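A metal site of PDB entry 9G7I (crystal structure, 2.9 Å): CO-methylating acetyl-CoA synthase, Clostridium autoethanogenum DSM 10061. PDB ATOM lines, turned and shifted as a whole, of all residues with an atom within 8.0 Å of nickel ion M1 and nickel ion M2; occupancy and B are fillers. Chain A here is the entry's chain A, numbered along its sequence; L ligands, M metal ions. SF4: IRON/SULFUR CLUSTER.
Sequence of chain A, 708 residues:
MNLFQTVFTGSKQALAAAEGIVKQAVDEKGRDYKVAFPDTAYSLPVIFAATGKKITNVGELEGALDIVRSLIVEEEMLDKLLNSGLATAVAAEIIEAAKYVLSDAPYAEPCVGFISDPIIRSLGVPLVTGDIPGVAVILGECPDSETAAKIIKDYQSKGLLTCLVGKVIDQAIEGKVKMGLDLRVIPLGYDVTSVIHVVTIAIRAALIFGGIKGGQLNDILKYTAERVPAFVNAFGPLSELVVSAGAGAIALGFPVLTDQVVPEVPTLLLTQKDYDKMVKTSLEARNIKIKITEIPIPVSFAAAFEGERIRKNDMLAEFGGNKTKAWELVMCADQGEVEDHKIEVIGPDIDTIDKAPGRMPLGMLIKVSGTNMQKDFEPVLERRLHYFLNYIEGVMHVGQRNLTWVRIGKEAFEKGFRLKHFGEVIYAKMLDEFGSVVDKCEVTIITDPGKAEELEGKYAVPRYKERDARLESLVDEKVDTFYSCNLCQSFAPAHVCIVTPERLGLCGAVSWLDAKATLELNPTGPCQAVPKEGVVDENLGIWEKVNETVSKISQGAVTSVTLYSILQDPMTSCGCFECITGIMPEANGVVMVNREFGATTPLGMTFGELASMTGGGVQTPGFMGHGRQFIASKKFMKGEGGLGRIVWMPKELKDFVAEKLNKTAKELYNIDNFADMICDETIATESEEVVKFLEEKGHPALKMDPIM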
ATOM      1  N   ARG A 383      15.658 -28.203  22.125  1.00  0.00           N
ATOM      2  CA  ARG A 383      14.929 -27.188  21.318  1.00  0.00           C
ATOM      3  C   ARG A 383      14.505 -26.036  22.239  1.00  0.00           C
ATOM      4  O   ARG A 383      14.727 -24.876  21.864  1.00  0.00           O
ATOM      5  CB  ARG A 383      13.710 -27.815  20.642  1.00  0.00           C
ATOM      6  CG  ARG A 383      12.823 -26.815  19.905  1.00  0.00           C
ATOM      7  CD  ARG A 383      13.542 -26.172  18.731  1.00  0.00           C
ATOM      8  NE  ARG A 383      12.763 -25.095  18.139  1.00  0.00           N
ATOM      9  CZ  ARG A 383      13.298 -24.052  17.509  1.00  0.00           C
ATOM     10  NH1 ARG A 383      14.613 -23.934  17.414  1.00  0.00           N
ATOM     11  NH2 ARG A 383      12.509 -23.127  16.985  1.00  0.00           N
ATOM     12  N   HIS A 386      16.766 -22.904  22.962  1.00  0.00           N
ATOM     13  CA  HIS A 386      16.737 -21.816  21.979  1.00  0.00           C
ATOM     14  C   HIS A 386      15.759 -20.729  22.414  1.00  0.00           C
ATOM     15  O   HIS A 386      16.062 -19.541  22.295  1.00  0.00           O
ATOM     16  CB  HIS A 386      16.372 -22.375  20.586  1.00  0.00           C
ATOM     17  CG  HIS A 386      15.700 -21.404  19.663  1.00  0.00           C
ATOM     18  ND1 HIS A 386      16.427 -20.430  18.988  1.00  0.00           N
ATOM     19  CD2 HIS A 386      14.409 -21.285  19.312  1.00  0.00           C
ATOM     20  CE1 HIS A 386      15.547 -19.763  18.263  1.00  0.00           C
ATOM     21  NE2 HIS A 386      14.311 -20.242  18.423  1.00  0.00           N
ATOM     22  N   TYR A 387      14.584 -21.131  22.913  1.00  0.00           N
ATOM     23  CA  TYR A 387      13.562 -20.180  23.357  1.00  0.00           C
ATOM     24  C   TYR A 387      13.964 -19.493  24.662  1.00  0.00           C
ATOM     25  O   TYR A 387      13.842 -18.276  24.762  1.00  0.00           O
ATOM     26  CB  TYR A 387      12.201 -20.888  23.500  1.00  0.00           C
ATOM     27  CG  TYR A 387      11.664 -21.401  22.179  1.00  0.00           C
ATOM     28  CD1 TYR A 387      12.070 -22.629  21.679  1.00  0.00           C
ATOM     29  CD2 TYR A 387      10.771 -20.652  21.427  1.00  0.00           C
ATOM     30  CE1 TYR A 387      11.595 -23.100  20.465  1.00  0.00           C
ATOM     31  CE2 TYR A 387      10.286 -21.121  20.204  1.00  0.00           C
ATOM     32  CZ  TYR A 387      10.713 -22.342  19.722  1.00  0.00           C
ATOM     33  OH  TYR A 387      10.248 -22.824  18.517  1.00  0.00           O
ATOM     34  N   CYS A 485       3.398 -28.800  13.887  1.00  0.00           N
ATOM     35  CA  CYS A 485       3.866 -27.873  14.913  1.00  0.00           C
ATOM     36  C   CYS A 485       3.452 -26.446  14.567  1.00  0.00           C
ATOM     37  O   CYS A 485       3.499 -26.066  13.390  1.00  0.00           O
ATOM     38  CB  CYS A 485       5.378 -27.981  15.089  1.00  0.00           C
ATOM     39  SG  CYS A 485       6.066 -26.767  16.258  1.00  0.00           S
ATOM     40  N   LEU A 487       4.578 -23.719  16.808  1.00  0.00           N
ATOM     41  CA  LEU A 487       5.359 -22.912  17.740  1.00  0.00           C
ATOM     42  C   LEU A 487       5.891 -21.656  17.045  1.00  0.00           C
ATOM     43  O   LEU A 487       5.941 -20.588  17.661  1.00  0.00           O
ATOM     44  CB  LEU A 487       6.514 -23.756  18.332  1.00  0.00           C
ATOM     45  CG  LEU A 487       6.966 -23.458  19.763  1.00  0.00           C
ATOM     46  CD1 LEU A 487       5.788 -23.326  20.738  1.00  0.00           C
ATOM     47  CD2 LEU A 487       7.939 -24.542  20.251  1.00  0.00           C
ATOM     48  N   CYS A 488       6.184 -21.752  15.750  1.00  0.00           N
ATOM     49  CA  CYS A 488       6.693 -20.583  14.984  1.00  0.00           C
ATOM     50  C   CYS A 488       5.548 -19.615  14.655  1.00  0.00           C
ATOM     51  O   CYS A 488       5.831 -18.576  14.021  1.00  0.00           O
ATOM     52  CB  CYS A 488       7.332 -21.035  13.686  1.00  0.00           C
ATOM     53  SG  CYS A 488       8.990 -21.743  13.928  1.00  0.00           S
ATOM     54  N   GLN A 489       4.325 -19.940  15.069  1.00  0.00           N
ATOM     55  CA  GLN A 489       3.180 -19.092  14.747  1.00  0.00           C
ATOM     56  C   GLN A 489       3.208 -17.753  15.522  1.00  0.00           C
ATOM     57  O   GLN A 489       2.381 -16.889  15.269  1.00  0.00           O
ATOM     58  CB  GLN A 489       1.863 -19.848  15.016  1.00  0.00           C
ATOM     59  CG  GLN A 489       0.699 -19.390  14.133  1.00  0.00           C
ATOM     60  CD  GLN A 489      -0.536 -20.252  14.294  1.00  0.00           C
ATOM     61  OE1 GLN A 489      -0.481 -21.363  14.812  1.00  0.00           O
ATOM     62  NE2 GLN A 489      -1.674 -19.745  13.852  1.00  0.00           N
ATOM     63  N   PHE A 491       5.540 -15.454  15.296  1.00  0.00           N
ATOM     64  CA  PHE A 491       5.947 -14.441  14.312  1.00  0.00           C
ATOM     65  C   PHE A 491       5.246 -14.665  12.970  1.00  0.00           C
ATOM     66  O   PHE A 491       4.798 -13.692  12.353  1.00  0.00           O
ATOM     67  CB  PHE A 491       7.479 -14.413  14.140  1.00  0.00           C
ATOM     68  CG  PHE A 491       8.165 -15.736  13.909  1.00  0.00           C
ATOM     69  CD1 PHE A 491       8.446 -16.579  14.961  1.00  0.00           C
ATOM     70  CD2 PHE A 491       8.606 -16.089  12.647  1.00  0.00           C
ATOM     71  CE1 PHE A 491       9.116 -17.780  14.755  1.00  0.00           C
ATOM     72  CE2 PHE A 491       9.267 -17.288  12.442  1.00  0.00           C
ATOM     73  CZ  PHE A 491       9.528 -18.120  13.495  1.00  0.00           C
ATOM     74  N   ALA A 492       5.138 -15.922  12.513  1.00  0.00           N
ATOM     75  CA  ALA A 492       4.463 -16.251  11.256  1.00  0.00           C
ATOM     76  C   ALA A 492       3.026 -16.713  11.541  1.00  0.00           C
ATOM     77  O   ALA A 492       2.821 -17.903  11.774  1.00  0.00           O
ATOM     78  CB  ALA A 492       5.208 -17.359  10.536  1.00  0.00           C
ATOM     79  N   HIS A 495       1.893 -20.039   9.645  1.00  0.00           N
ATOM     80  CA  HIS A 495       2.848 -21.139   9.482  1.00  0.00           C
ATOM     81  C   HIS A 495       2.426 -22.367  10.260  1.00  0.00           C
ATOM     82  O   HIS A 495       2.256 -22.303  11.487  1.00  0.00           O
ATOM     83  CB  HIS A 495       4.252 -20.708   9.921  1.00  0.00           C
ATOM     84  CG  HIS A 495       5.271 -21.795   9.784  1.00  0.00           C
ATOM     85  ND1 HIS A 495       5.875 -22.065   8.574  1.00  0.00           N
ATOM     86  CD2 HIS A 495       5.742 -22.665  10.712  1.00  0.00           C
ATOM     87  CE1 HIS A 495       6.707 -23.069   8.803  1.00  0.00           C
ATOM     88  NE2 HIS A 495       6.653 -23.470  10.069  1.00  0.00           N
ATOM     89  N   CYS A 497       3.961 -26.068  10.472  1.00  0.00           N
ATOM     90  CA  CYS A 497       5.069 -26.936   9.994  1.00  0.00           C
ATOM     91  C   CYS A 497       4.725 -28.421  10.099  1.00  0.00           C
ATOM     92  O   CYS A 497       4.681 -28.931  11.231  1.00  0.00           O
ATOM     93  CB  CYS A 497       6.360 -26.661  10.777  1.00  0.00           C
ATOM     94  SG  CYS A 497       7.867 -27.242   9.959  1.00  0.00           S
ATOM     95  N   GLY A 505      11.386 -30.540  10.590  1.00  0.00           N
ATOM     96  CA  GLY A 505      10.965 -29.177  10.965  1.00  0.00           C
ATOM     97  C   GLY A 505      11.925 -28.158  10.396  1.00  0.00           C
ATOM     98  O   GLY A 505      13.150 -28.338  10.590  1.00  0.00           O
ATOM     99  N   LEU A 506      11.416 -27.148   9.714  1.00  0.00           N
ATOM    100  CA  LEU A 506      12.276 -26.158   9.061  1.00  0.00           C
ATOM    101  C   LEU A 506      13.362 -25.644  10.014  1.00  0.00           C
ATOM    102  O   LEU A 506      14.414 -25.190   9.565  1.00  0.00           O
ATOM    103  CB  LEU A 506      11.469 -24.978   8.494  1.00  0.00           C
ATOM    104  CG  LEU A 506      10.228 -25.307   7.646  1.00  0.00           C
ATOM    105  CD1 LEU A 506       9.683 -24.063   6.983  1.00  0.00           C
ATOM    106  CD2 LEU A 506      10.522 -26.363   6.586  1.00  0.00           C
ATOM    107  N   CYS A 507      13.143 -25.717  11.320  1.00  0.00           N
ATOM    108  CA  CYS A 507      14.199 -25.148  12.207  1.00  0.00           C
ATOM    109  C   CYS A 507      15.408 -26.077  12.252  1.00  0.00           C
ATOM    110  O   CYS A 507      16.508 -25.593  12.592  1.00  0.00           O
ATOM    111  CB  CYS A 507      13.675 -24.921  13.611  1.00  0.00           C
ATOM    112  SG  CYS A 507      13.181 -26.464  14.406  1.00  0.00           S
ATOM    113  N   GLY A 508      15.233 -27.349  11.880  1.00  0.00           N
ATOM    114  CA  GLY A 508      16.351 -28.307  11.820  1.00  0.00           C
ATOM    115  C   GLY A 508      16.457 -29.137  13.094  1.00  0.00           C
ATOM    116  O   GLY A 508      17.203 -30.128  13.089  1.00  0.00           O
ATOM    117  N   THR A 572       4.513 -23.611   3.692  1.00  0.00           N
ATOM    118  CA  THR A 572       4.912 -22.273   4.151  1.00  0.00           C
ATOM    119  C   THR A 572       6.222 -22.311   4.935  1.00  0.00           C
ATOM    120  O   THR A 572       6.563 -23.333   5.527  1.00  0.00           O
ATOM    121  CB  THR A 572       3.774 -21.639   4.976  1.00  0.00           C
ATOM    122  OG1 THR A 572       3.346 -22.570   5.973  1.00  0.00           O
ATOM    123  CG2 THR A 572       2.589 -21.210   4.124  1.00  0.00           C
ATOM    124  N   SER A 573       6.967 -21.201   4.914  1.00  0.00           N
ATOM    125  CA  SER A 573       8.247 -21.084   5.613  1.00  0.00           C
ATOM    126  C   SER A 573       8.118 -20.068   6.771  1.00  0.00           C
ATOM    127  O   SER A 573       7.287 -19.167   6.700  1.00  0.00           O
ATOM    128  CB  SER A 573       9.359 -20.677   4.647  1.00  0.00           C
ATOM    129  OG  SER A 573       9.444 -21.589   3.565  1.00  0.00           O
ATOM    130  N   CYS A 574       8.922 -20.221   7.836  1.00  0.00           N
ATOM    131  CA  CYS A 574       8.849 -19.351   9.007  1.00  0.00           C
ATOM    132  C   CYS A 574       9.989 -18.303   9.088  1.00  0.00           C
ATOM    133  O   CYS A 574       9.784 -17.158   8.681  1.00  0.00           O
ATOM    134  CB  CYS A 574       8.773 -20.192  10.283  1.00  0.00           C
ATOM    135  SG  CYS A 574       9.867 -21.632  10.293  1.00  0.00           S
ATOM    136  N   GLY A 575      11.164 -18.685   9.601  1.00  0.00           N
ATOM    137  CA  GLY A 575      12.283 -17.766   9.721  1.00  0.00           C
ATOM    138  C   GLY A 575      13.522 -18.338  10.395  1.00  0.00           C
ATOM    139  O   GLY A 575      14.530 -17.640  10.546  1.00  0.00           O
ATOM    140  N   CYS A 576      13.463 -19.607  10.817  1.00  0.00           N
ATOM    141  CA  CYS A 576      14.567 -20.306  11.487  1.00  0.00           C
ATOM    142  C   CYS A 576      15.324 -21.250  10.559  1.00  0.00           C
ATOM    143  O   CYS A 576      16.167 -22.009  11.034  1.00  0.00           O
ATOM    144  CB  CYS A 576      14.022 -21.058  12.697  1.00  0.00           C
ATOM    145  SG  CYS A 576      12.626 -22.144  12.310  1.00  0.00           S
ATOM    146  N   PHE A 577      15.052 -21.157   9.256  1.00  0.00           N
ATOM    147  CA  PHE A 577      15.709 -22.040   8.257  1.00  0.00           C
ATOM    148  C   PHE A 577      17.207 -21.739   8.205  1.00  0.00           C
ATOM    149  O   PHE A 577      17.581 -20.559   8.100  1.00  0.00           O
ATOM    150  CB  PHE A 577      15.056 -21.876   6.881  1.00  0.00           C
ATOM    151  CG  PHE A 577      14.523 -20.507   6.511  1.00  0.00           C
ATOM    152  CD1 PHE A 577      15.381 -19.472   6.180  1.00  0.00           C
ATOM    153  CD2 PHE A 577      13.163 -20.266   6.448  1.00  0.00           C
ATOM    154  CE1 PHE A 577      14.897 -18.230   5.824  1.00  0.00           C
ATOM    155  CE2 PHE A 577      12.670 -19.022   6.093  1.00  0.00           C
ATOM    156  CZ  PHE A 577      13.536 -17.999   5.771  1.00  0.00           C
ATOM    157  N   GLU A 578      18.044 -22.771   8.272  1.00  0.00           N
ATOM    158  CA  GLU A 578      19.511 -22.537   8.160  1.00  0.00           C
ATOM    159  C   GLU A 578      19.901 -22.448   6.682  1.00  0.00           C
ATOM    160  O   GLU A 578      20.823 -21.672   6.360  1.00  0.00           O
ATOM    161  CB  GLU A 578      20.257 -23.644   8.903  1.00  0.00           C
ATOM    162  CG  GLU A 578      21.710 -23.734   8.493  1.00  0.00           C
ATOM    163  CD  GLU A 578      22.621 -22.610   8.952  1.00  0.00           C
ATOM    164  OE1 GLU A 578      22.783 -22.449  10.169  1.00  0.00           O
ATOM    165  OE2 GLU A 578      23.195 -21.918   8.080  1.00  0.00           O
ATOM    166  N   ARG A 595      22.986 -19.868   6.152  1.00  0.00           N
ATOM    167  CA  ARG A 595      22.983 -18.626   6.917  1.00  0.00           C
ATOM    168  C   ARG A 595      24.387 -18.040   7.129  1.00  0.00           C
ATOM    169  O   ARG A 595      24.531 -16.831   7.301  1.00  0.00           O
ATOM    170  CB  ARG A 595      22.300 -18.844   8.280  1.00  0.00           C
ATOM    171  CG  ARG A 595      21.780 -17.556   8.930  1.00  0.00           C
ATOM    172  CD  ARG A 595      21.391 -17.736  10.395  1.00  0.00           C
ATOM    173  NE  ARG A 595      20.189 -18.571  10.564  1.00  0.00           N
ATOM    174  CZ  ARG A 595      20.188 -19.873  10.841  1.00  0.00           C
ATOM    175  NH1 ARG A 595      21.339 -20.537  10.977  1.00  0.00           N
ATOM    176  NH2 ARG A 595      19.044 -20.523  10.981  1.00  0.00           N
ATOM    177  N   THR A 614      11.151 -16.193   1.446  1.00  0.00           N
ATOM    178  CA  THR A 614      10.636 -17.545   1.796  1.00  0.00           C
ATOM    179  C   THR A 614       9.733 -17.557   3.029  1.00  0.00           C
ATOM    180  O   THR A 614       8.631 -18.126   2.938  1.00  0.00           O
ATOM    181  CB  THR A 614      11.860 -18.439   2.012  1.00  0.00           C
ATOM    182  OG1 THR A 614      12.616 -17.893   3.098  1.00  0.00           O
ATOM    183  CG2 THR A 614      12.720 -18.553   0.778  1.00  0.00           C
ATOM    184  N   GLY A 615      10.183 -16.950   4.128  1.00  0.00           N
ATOM    185  CA  GLY A 615       9.420 -16.997   5.391  1.00  0.00           C
ATOM    186  C   GLY A 615       8.167 -16.156   5.426  1.00  0.00           C
ATOM    187  O   GLY A 615       7.643 -15.820   4.347  1.00  0.00           O
ATOM    188  N   GLY A 616       7.711 -15.821   6.629  1.00  0.00           N
ATOM    189  CA  GLY A 616       6.495 -15.047   6.861  1.00  0.00           C
ATOM    190  C   GLY A 616       5.206 -15.840   6.856  1.00  0.00           C
ATOM    191  O   GLY A 616       4.120 -15.257   6.914  1.00  0.00           O
ATOM    192  N   GLY A 625      12.512 -22.780   2.627  1.00  0.00           N
ATOM    193  CA  GLY A 625      13.460 -22.838   3.735  1.00  0.00           C
ATOM    194  C   GLY A 625      13.531 -24.234   4.315  1.00  0.00           C
ATOM    195  O   GLY A 625      12.497 -24.885   4.457  1.00  0.00           O
ATOM    196  N   HIS A 626      14.733 -24.715   4.633  1.00  0.00           N
ATOM    197  CA  HIS A 626      14.916 -26.071   5.167  1.00  0.00           C
ATOM    198  C   HIS A 626      16.220 -26.180   5.979  1.00  0.00           C
ATOM    199  O   HIS A 626      17.071 -25.301   5.925  1.00  0.00           O
ATOM    200  CB  HIS A 626      14.935 -27.076   4.006  1.00  0.00           C
ATOM    201  CG  HIS A 626      15.962 -26.759   2.963  1.00  0.00           C
ATOM    202  ND1 HIS A 626      17.201 -27.369   2.975  1.00  0.00           N
ATOM    203  CD2 HIS A 626      15.918 -25.890   1.936  1.00  0.00           C
ATOM    204  CE1 HIS A 626      17.867 -26.854   1.951  1.00  0.00           C
ATOM    205  NE2 HIS A 626      17.125 -25.961   1.292  1.00  0.00           N
HETATM  206 FE1  SF4 L   1       8.222 -26.369  14.951  1.00  0.00          FE
HETATM  207 FE2  SF4 L   1       8.762 -26.244  12.402  1.00  0.00          FE
HETATM  208 FE3  SF4 L   1      10.739 -26.239  14.164  1.00  0.00          FE
HETATM  209 FE4  SF4 L   1       9.132 -24.140  13.936  1.00  0.00          FE
HETATM  210  S1  SF4 L   1      10.598 -24.872  12.325  1.00  0.00           S
HETATM  211  S2  SF4 L   1       9.843 -25.045  15.920  1.00  0.00           S
HETATM  212  S3  SF4 L   1       7.091 -25.058  13.447  1.00  0.00           S
HETATM  213  S4  SF4 L   1       9.334 -27.998  13.761  1.00  0.00           S
HETATM  214 NI    NI M   1      10.590 -21.963  12.191  1.00  0.00          NI
HETATM  215 NI    NI M   2      11.758 -20.381  10.460  1.00  0.00          NI
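An iron atom (FE4) of the ligand is bound by the side-chain sulfur of Cys 488 (2.4 Å). A sulfur (S1) of the ligand sits close to the backbone NH of Cys 507. An iron atom (FE3) of the ligand is bound by the side-chain sulfur (SG) of Cys 507. NE2 of His 495 sits close to S3 of the ligand (3.8 Å). A sulfur (S1) of the ligand lies close to the backbone NH of Leu 506 (3.6 Å). The guanidinium group of Arg 383 lies close to a sulfur (S2) of the ligand. The side-chain sulfur of Cys 497 is bound to an iron atom (FE2) of the ligand (2.8 Å). The side-chain hydroxyl of Tyr 387 lies close to a sulfur (S2) of the ligand, at 3.4 Å. FE1 of the ligand is bound by SG of Cys 485 (2.6 Å).
N of Cys 507 sits close to SG of Cys 576, 3.7 Å away. The guanidinium group of Arg 595 lies within hydrogen-bond range of the backbone carbonyl oxygen of Cys 576, 3.2 Å away. The side-chain sulfur of Cys 574 lies close to a ring nitrogen (NE2) of His 495 (3.7 Å). The backbone carbonyl oxygen (O) of Cys 574 sits at hydrogen-bond distance from the backbone NH (N) of Gly 616, 3.2 Å away. The guanidinium group (NH2) of Arg 595 sits at hydrogen-bond distance from the backbone carbonyl oxygen (O) of Phe 577.
Three residues have an atom within 4 Å of nickel ion M1: Cys 488, Cys 574 and Cys 576. Along chain A the residues within 4 Å of nickel ion M1 span positions 488 to 576.
Residues that only touch nickel ion M2: Phe 577 (3.6 Å). Within 4 Å of nickel ion M2: Cys 574, Gly 575, Cys 576 and Phe 577. The nearest printed residue that does not touch nickel ion M2 is Phe 491 (4.4 Å).
Nickel ion M1 is bound by SG of Cys 576 (2.0 Å). SG of Cys 574 is bound to nickel ion M1 (2.1 Å). Nickel ion M1 is bound by the side-chain sulfur (SG) of Cys 488 (2.4 Å). Slightly farther from nickel ion M1 lies S1 of the ligand (2.9 Å).
Nickel ion M2 is bound by N of Cys 576 (1.9 Å). N of Gly 575 binds nickel ion M2 (2.0 Å). Nickel ion M2 is bound by the side-chain sulfur (SG) of Cys 574 (2.3 Å). Nickel ion M2 is bound by the side-chain sulfur (SG) of Cys 576, at 2.7 Å. Nickel ion M2 has four donor atoms within binding distance.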
